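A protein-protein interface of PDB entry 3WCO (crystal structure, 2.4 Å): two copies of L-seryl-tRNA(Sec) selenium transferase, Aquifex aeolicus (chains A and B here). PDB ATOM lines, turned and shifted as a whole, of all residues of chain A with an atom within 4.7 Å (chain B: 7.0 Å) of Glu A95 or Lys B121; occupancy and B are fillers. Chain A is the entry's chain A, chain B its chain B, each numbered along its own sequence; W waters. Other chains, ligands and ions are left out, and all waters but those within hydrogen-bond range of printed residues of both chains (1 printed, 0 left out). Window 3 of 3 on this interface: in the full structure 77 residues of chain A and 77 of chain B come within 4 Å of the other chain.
OD1 of Asn A91 lies within hydrogen-bond range of NZ of Lys B121.
The side-chain carboxylate (OE1) of Glu A95 lies within salt-bridge range of the side-chain amino group (NZ) of Lys B121, 3.8 Å away.
N of Ile A250 is in hydrogen-bond range of OD1 of Asn A248 (2.9 Å).
ND2 of Asn A91 sits at hydrogen-bond distance from O of Ser A122.
The side-chain amide oxygen of Asn A91 lies within hydrogen-bond range of the side-chain amide nitrogen of Asn A248.
Asn A248 touches Lys B121.
Pro A249 touches Asp B117 (CB to CB, 3.98 Å).
Ile B118 touches Pro A249.
Lys B121 touches Pro A249.
Ile A250 touches Phe B87.
Ile A250 touches Lys B121.
Of the printed residues of chain B, Glu A95 touches Lys B121.
Lys B121 touches just these residues of chain A: Asn A91 (3.2 Å), Glu A95 (3.8 Å), Asn A248 (3.4 Å), Pro A249 (3.5 Å) and Ile A250 (3.8 Å).
Printed residues of chain B within 4 Å of Asn A248: Lys B121.
Printed residues of chain B within 4 Å of Ile A250: Phe B87 and Lys B121.
Printed residues of chain B within 4 Å of Asn A91: Lys B121 (3.2 Å).
Among the printed residues, Asp or Glu carboxylates within 4 Å of a Lys or Arg side-chain nitrogen of the other chain: Glu A95 with Lys B121 (3.8 Å).
Positions printed for both chains: 91, 122, 123 and 124.
Of the 8 pairs that touch across the chains among the printed residues, none has its exchanged pair printed and touching as well.
Water W1 lies within hydrogen-bond range of OE2 of Glu A95 (2.6 Å), ND2 of Asn A91 (2.8 Å) and O of Lys B121 (3.0 Å).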
ATOM      1  N   LEU A  90       1.066  22.028  -1.113  1.00  0.00           N
ATOM      2  CA  LEU A  90       0.556  23.397  -1.117  1.00  0.00           C
ATOM      3  C   LEU A  90      -0.573  23.596  -2.142  1.00  0.00           C
ATOM      4  O   LEU A  90      -1.666  24.059  -1.791  1.00  0.00           O
ATOM      5  CB  LEU A  90       1.680  24.401  -1.362  1.00  0.00           C
ATOM      6  CG  LEU A  90       2.402  24.937  -0.125  1.00  0.00           C
ATOM      7  CD1 LEU A  90       2.841  23.831   0.816  1.00  0.00           C
ATOM      8  CD2 LEU A  90       3.600  25.739  -0.568  1.00  0.00           C
ATOM      9  N   ASN A  91      -0.326  23.236  -3.400  1.00  0.00           N
ATOM     10  CA  ASN A  91      -1.347  23.451  -4.431  1.00  0.00           C
ATOM     11  C   ASN A  91      -2.648  22.713  -4.107  1.00  0.00           C
ATOM     12  O   ASN A  91      -3.743  23.255  -4.283  1.00  0.00           O
ATOM     13  CB  ASN A  91      -0.846  23.101  -5.829  1.00  0.00           C
ATOM     14  CG  ASN A  91      -1.950  23.187  -6.879  1.00  0.00           C
ATOM     15  OD1 ASN A  91      -2.748  22.258  -7.043  1.00  0.00           O
ATOM     16  ND2 ASN A  91      -2.004  24.307  -7.589  1.00  0.00           N
ATOM     17  N   LEU A  93      -3.795  21.663  -0.961  1.00  0.00           N
ATOM     18  CA  LEU A  93      -4.520  22.041   0.251  1.00  0.00           C
ATOM     19  C   LEU A  93      -4.788  23.534   0.393  1.00  0.00           C
ATOM     20  O   LEU A  93      -5.638  23.933   1.187  1.00  0.00           O
ATOM     21  CB  LEU A  93      -3.795  21.529   1.498  1.00  0.00           C
ATOM     22  CG  LEU A  93      -3.600  20.017   1.578  1.00  0.00           C
ATOM     23  CD1 LEU A  93      -2.882  19.590   2.870  1.00  0.00           C
ATOM     24  CD2 LEU A  93      -4.927  19.319   1.435  1.00  0.00           C
ATOM     25  N   ALA A  94      -4.094  24.360  -0.384  1.00  0.00           N
ATOM     26  CA  ALA A  94      -4.122  25.802  -0.131  1.00  0.00           C
ATOM     27  C   ALA A  94      -4.091  26.692  -1.370  1.00  0.00           C
ATOM     28  O   ALA A  94      -3.616  27.830  -1.301  1.00  0.00           O
ATOM     29  CB  ALA A  94      -2.982  26.185   0.807  1.00  0.00           C
ATOM     30  N   GLU A  95      -4.589  26.184  -2.492  1.00  0.00           N
ATOM     31  CA  GLU A  95      -4.688  27.008  -3.682  1.00  0.00           C
ATOM     32  C   GLU A  95      -5.596  28.198  -3.388  1.00  0.00           C
ATOM     33  O   GLU A  95      -6.712  28.027  -2.885  1.00  0.00           O
ATOM     34  CB  GLU A  95      -5.252  26.199  -4.843  1.00  0.00           C
ATOM     35  CG  GLU A  95      -4.942  26.802  -6.206  1.00  0.00           C
ATOM     36  CD  GLU A  95      -5.525  25.994  -7.352  1.00  0.00           C
ATOM     37  OE1 GLU A  95      -6.382  25.116  -7.098  1.00  0.00           O
ATOM     38  OE2 GLU A  95      -5.124  26.239  -8.508  1.00  0.00           O
ATOM     39  N   GLY A  96      -5.097  29.397  -3.680  1.00  0.00           N
ATOM     40  CA  GLY A  96      -5.830  30.630  -3.447  1.00  0.00           C
ATOM     41  C   GLY A  96      -6.113  30.912  -1.979  1.00  0.00           C
ATOM     42  O   GLY A  96      -7.054  31.633  -1.641  1.00  0.00           O
ATOM     43  N   LYS A  97      -5.308  30.334  -1.097  1.00  0.00           N
ATOM     44  CA  LYS A  97      -5.503  30.525   0.334  1.00  0.00           C
ATOM     45  C   LYS A  97      -4.154  30.657   1.047  1.00  0.00           C
ATOM     46  O   LYS A  97      -3.099  30.579   0.413  1.00  0.00           O
ATOM     47  CB  LYS A  97      -6.330  29.377   0.929  1.00  0.00           C
ATOM     48  CG  LYS A  97      -7.803  29.381   0.526  1.00  0.00           C
ATOM     49  CD  LYS A  97      -8.562  28.198   1.127  1.00  0.00           C
ATOM     50  CE  LYS A  97      -9.129  28.510   2.511  1.00  0.00           C
ATOM     51  NZ  LYS A  97      -9.677  27.296   3.202  1.00  0.00           N
ATOM     52  N   SER A 122       2.856  27.775  -6.365  1.00  0.00           N
ATOM     53  CA  SER A 122       1.950  26.647  -6.137  1.00  0.00           C
ATOM     54  C   SER A 122       0.481  27.072  -6.212  1.00  0.00           C
ATOM     55  O   SER A 122      -0.410  26.222  -6.342  1.00  0.00           O
ATOM     56  CB  SER A 122       2.222  26.027  -4.774  1.00  0.00           C
ATOM     57  OG  SER A 122       1.766  26.897  -3.756  1.00  0.00           O
ATOM     58  N   GLY A 123       0.236  28.381  -6.119  1.00  0.00           N
ATOM     59  CA  GLY A 123      -1.113  28.916  -6.066  1.00  0.00           C
ATOM     60  C   GLY A 123      -1.479  29.280  -4.642  1.00  0.00           C
ATOM     61  O   GLY A 123      -2.575  29.772  -4.367  1.00  0.00           O
ATOM     62  N   ALA A 124      -0.552  29.025  -3.728  1.00  0.00           N
ATOM     63  CA  ALA A 124      -0.770  29.335  -2.324  1.00  0.00           C
ATOM     64  C   ALA A 124      -0.259  30.738  -2.018  1.00  0.00           C
ATOM     65  O   ALA A 124       0.719  31.204  -2.619  1.00  0.00           O
ATOM     66  CB  ALA A 124      -0.078  28.302  -1.425  1.00  0.00           C
ATOM     67  N   ASN A 248      -5.229  15.151  -7.107  1.00  0.00           N
ATOM     68  CA  ASN A 248      -4.795  16.352  -7.788  1.00  0.00           C
ATOM     69  C   ASN A 248      -4.138  15.945  -9.091  1.00  0.00           C
ATOM     70  O   ASN A 248      -3.090  15.301  -9.083  1.00  0.00           O
ATOM     71  CB  ASN A 248      -3.811  17.123  -6.931  1.00  0.00           C
ATOM     72  CG  ASN A 248      -3.469  18.479  -7.511  1.00  0.00           C
ATOM     73  OD1 ASN A 248      -3.427  18.652  -8.730  1.00  0.00           O
ATOM     74  ND2 ASN A 248      -3.218  19.464  -6.626  1.00  0.00           N
ATOM     75  N   PRO A 249      -4.746  16.333 -10.219  1.00  0.00           N
ATOM     76  CA  PRO A 249      -4.237  15.918 -11.530  1.00  0.00           C
ATOM     77  C   PRO A 249      -2.766  16.274 -11.700  1.00  0.00           C
ATOM     78  O   PRO A 249      -2.061  15.602 -12.459  1.00  0.00           O
ATOM     79  CB  PRO A 249      -5.119  16.687 -12.525  1.00  0.00           C
ATOM     80  CG  PRO A 249      -5.807  17.757 -11.718  1.00  0.00           C
ATOM     81  CD  PRO A 249      -5.910  17.229 -10.319  1.00  0.00           C
ATOM     82  N   ILE A 250      -2.299  17.299 -10.993  1.00  0.00           N
ATOM     83  CA  ILE A 250      -0.878  17.635 -11.013  1.00  0.00           C
ATOM     84  C   ILE A 250      -0.008  16.440 -10.588  1.00  0.00           C
ATOM     85  O   ILE A 250       1.135  16.293 -11.053  1.00  0.00           O
ATOM     86  CB  ILE A 250      -0.597  18.878 -10.157  1.00  0.00           C
ATOM     87  CG1 ILE A 250      -1.321  20.073 -10.772  1.00  0.00           C
ATOM     88  CG2 ILE A 250       0.891  19.176 -10.061  1.00  0.00           C
ATOM     89  CD1 ILE A 250      -0.997  21.382 -10.114  1.00  0.00           C
ATOM     90  N   PHE B  87       2.286  20.684 -18.765  1.00  0.00           N
ATOM     91  CA  PHE B  87       1.954  21.531 -17.652  1.00  0.00           C
ATOM     92  C   PHE B  87       2.945  22.662 -17.601  1.00  0.00           C
ATOM     93  O   PHE B  87       2.564  23.833 -17.506  1.00  0.00           O
ATOM     94  CB  PHE B  87       2.042  20.712 -16.369  1.00  0.00           C
ATOM     95  CG  PHE B  87       1.767  21.497 -15.113  1.00  0.00           C
ATOM     96  CD1 PHE B  87       0.466  21.868 -14.774  1.00  0.00           C
ATOM     97  CD2 PHE B  87       2.807  21.831 -14.245  1.00  0.00           C
ATOM     98  CE1 PHE B  87       0.210  22.579 -13.592  1.00  0.00           C
ATOM     99  CE2 PHE B  87       2.559  22.543 -13.062  1.00  0.00           C
ATOM    100  CZ  PHE B  87       1.261  22.916 -12.737  1.00  0.00           C
ATOM    101  N   ASN B  91       2.111  26.490 -18.174  1.00  0.00           N
ATOM    102  CA  ASN B  91       2.278  27.390 -17.041  1.00  0.00           C
ATOM    103  C   ASN B  91       3.320  28.478 -17.315  1.00  0.00           C
ATOM    104  O   ASN B  91       3.151  29.645 -16.942  1.00  0.00           O
ATOM    105  CB  ASN B  91       2.619  26.635 -15.760  1.00  0.00           C
ATOM    106  CG  ASN B  91       2.821  27.579 -14.589  1.00  0.00           C
ATOM    107  OD1 ASN B  91       3.916  28.103 -14.388  1.00  0.00           O
ATOM    108  ND2 ASN B  91       1.747  27.849 -13.852  1.00  0.00           N
ATOM    109  N   ILE B 115      -4.748  14.351 -18.219  1.00  0.00           N
ATOM    110  CA  ILE B 115      -3.960  15.379 -18.875  1.00  0.00           C
ATOM    111  C   ILE B 115      -4.761  16.657 -19.144  1.00  0.00           C
ATOM    112  O   ILE B 115      -4.262  17.758 -18.861  1.00  0.00           O
ATOM    113  CB  ILE B 115      -3.353  14.899 -20.189  1.00  0.00           C
ATOM    114  CG1 ILE B 115      -2.634  13.557 -20.005  1.00  0.00           C
ATOM    115  CG2 ILE B 115      -2.455  15.974 -20.765  1.00  0.00           C
ATOM    116  CD1 ILE B 115      -1.330  13.630 -19.280  1.00  0.00           C
ATOM    117  N   PRO B 116      -5.992  16.533 -19.697  1.00  0.00           N
ATOM    118  CA  PRO B 116      -6.661  17.816 -19.962  1.00  0.00           C
ATOM    119  C   PRO B 116      -6.861  18.605 -18.676  1.00  0.00           C
ATOM    120  O   PRO B 116      -6.707  19.826 -18.689  1.00  0.00           O
ATOM    121  CB  PRO B 116      -8.011  17.417 -20.596  1.00  0.00           C
ATOM    122  CG  PRO B 116      -8.146  15.938 -20.401  1.00  0.00           C
ATOM    123  CD  PRO B 116      -6.760  15.384 -20.222  1.00  0.00           C
ATOM    124  N   ASP B 117      -7.148  17.913 -17.578  1.00  0.00           N
ATOM    125  CA  ASP B 117      -7.280  18.575 -16.280  1.00  0.00           C
ATOM    126  C   ASP B 117      -5.971  19.204 -15.765  1.00  0.00           C
ATOM    127  O   ASP B 117      -5.992  20.240 -15.111  1.00  0.00           O
ATOM    128  CB  ASP B 117      -7.863  17.604 -15.258  1.00  0.00           C
ATOM    129  CG  ASP B 117      -9.257  17.155 -15.629  1.00  0.00           C
ATOM    130  OD1 ASP B 117      -9.669  16.045 -15.227  1.00  0.00           O
ATOM    131  OD2 ASP B 117      -9.934  17.921 -16.344  1.00  0.00           O
ATOM    132  N   ILE B 118      -4.839  18.582 -16.071  1.00  0.00           N
ATOM    133  CA  ILE B 118      -3.538  19.158 -15.752  1.00  0.00           C
ATOM    134  C   ILE B 118      -3.380  20.510 -16.434  1.00  0.00           C
ATOM    135  O   ILE B 118      -2.893  21.477 -15.832  1.00  0.00           O
ATOM    136  CB  ILE B 118      -2.403  18.218 -16.197  1.00  0.00           C
ATOM    137  CG1 ILE B 118      -2.365  16.989 -15.285  1.00  0.00           C
ATOM    138  CG2 ILE B 118      -1.065  18.933 -16.212  1.00  0.00           C
ATOM    139  CD1 ILE B 118      -1.261  16.021 -15.617  1.00  0.00           C
ATOM    140  N   MET B 119      -3.806  20.576 -17.689  1.00  0.00           N
ATOM    141  CA  MET B 119      -3.754  21.816 -18.432  1.00  0.00           C
ATOM    142  C   MET B 119      -4.645  22.852 -17.780  1.00  0.00           C
ATOM    143  O   MET B 119      -4.348  24.042 -17.804  1.00  0.00           O
ATOM    144  CB  MET B 119      -4.215  21.571 -19.850  1.00  0.00           C
ATOM    145  CG  MET B 119      -3.352  20.575 -20.576  1.00  0.00           C
ATOM    146  SD  MET B 119      -3.998  20.233 -22.392  1.00  0.00           S
ATOM    147  CE  MET B 119      -4.208  22.076 -22.984  1.00  0.00           C
ATOM    148  N   LYS B 120      -5.742  22.401 -17.188  1.00  0.00           N
ATOM    149  CA  LYS B 120      -6.618  23.319 -16.471  1.00  0.00           C
ATOM    150  C   LYS B 120      -5.947  23.830 -15.193  1.00  0.00           C
ATOM    151  O   LYS B 120      -6.156  24.975 -14.802  1.00  0.00           O
ATOM    152  CB  LYS B 120      -7.958  22.656 -16.151  1.00  0.00           C
ATOM    153  CG  LYS B 120      -8.764  22.256 -17.377  1.00  0.00           C
ATOM    154  CD  LYS B 120     -10.161  21.818 -16.971  1.00  0.00           C
ATOM    155  CE  LYS B 120     -11.153  22.007 -18.111  1.00  0.00           C
ATOM    156  NZ  LYS B 120     -12.490  22.475 -17.627  1.00  0.00           N
ATOM    157  N   LYS B 121      -5.130  22.985 -14.564  1.00  0.00           N
ATOM    158  CA  LYS B 121      -4.430  23.353 -13.334  1.00  0.00           C
ATOM    159  C   LYS B 121      -3.211  24.207 -13.622  1.00  0.00           C
ATOM    160  O   LYS B 121      -2.645  24.780 -12.706  1.00  0.00           O
ATOM    161  CB  LYS B 121      -3.957  22.113 -12.561  1.00  0.00           C
ATOM    162  CG  LYS B 121      -5.054  21.184 -12.091  1.00  0.00           C
ATOM    163  CD  LYS B 121      -5.733  21.664 -10.821  1.00  0.00           C
ATOM    164  CE  LYS B 121      -4.821  21.578  -9.618  1.00  0.00           C
ATOM    165  NZ  LYS B 121      -5.623  21.602  -8.368  1.00  0.00           N
ATOM    166  N   SER B 122      -2.806  24.286 -14.890  1.00  0.00           N
ATOM    167  CA  SER B 122      -1.565  24.962 -15.244  1.00  0.00           C
ATOM    168  C   SER B 122      -1.729  26.453 -15.019  1.00  0.00           C
ATOM    169  O   SER B 122      -0.753  27.196 -15.012  1.00  0.00           O
ATOM    170  CB  SER B 122      -1.224  24.715 -16.706  1.00  0.00           C
ATOM    171  OG  SER B 122      -2.009  25.552 -17.529  1.00  0.00           O
ATOM    172  N   GLY B 123      -2.975  26.884 -14.838  1.00  0.00           N
ATOM    173  CA  GLY B 123      -3.275  28.290 -14.680  1.00  0.00           C
ATOM    174  C   GLY B 123      -3.445  28.986 -16.013  1.00  0.00           C
ATOM    175  O   GLY B 123      -3.565  30.212 -16.073  1.00  0.00           O
ATOM    176  N   ALA B 124      -3.445  28.211 -17.095  1.00  0.00           N
ATOM    177  CA  ALA B 124      -3.737  28.793 -18.398  1.00  0.00           C
ATOM    178  C   ALA B 124      -5.240  28.771 -18.602  1.00  0.00           C
ATOM    179  O   ALA B 124      -5.936  27.898 -18.081  1.00  0.00           O
ATOM    180  CB  ALA B 124      -3.022  28.044 -19.520  1.00  0.00           C
HETATM  181  O   HOH W   1      -3.527  24.801  -9.887  1.00  0.00           O
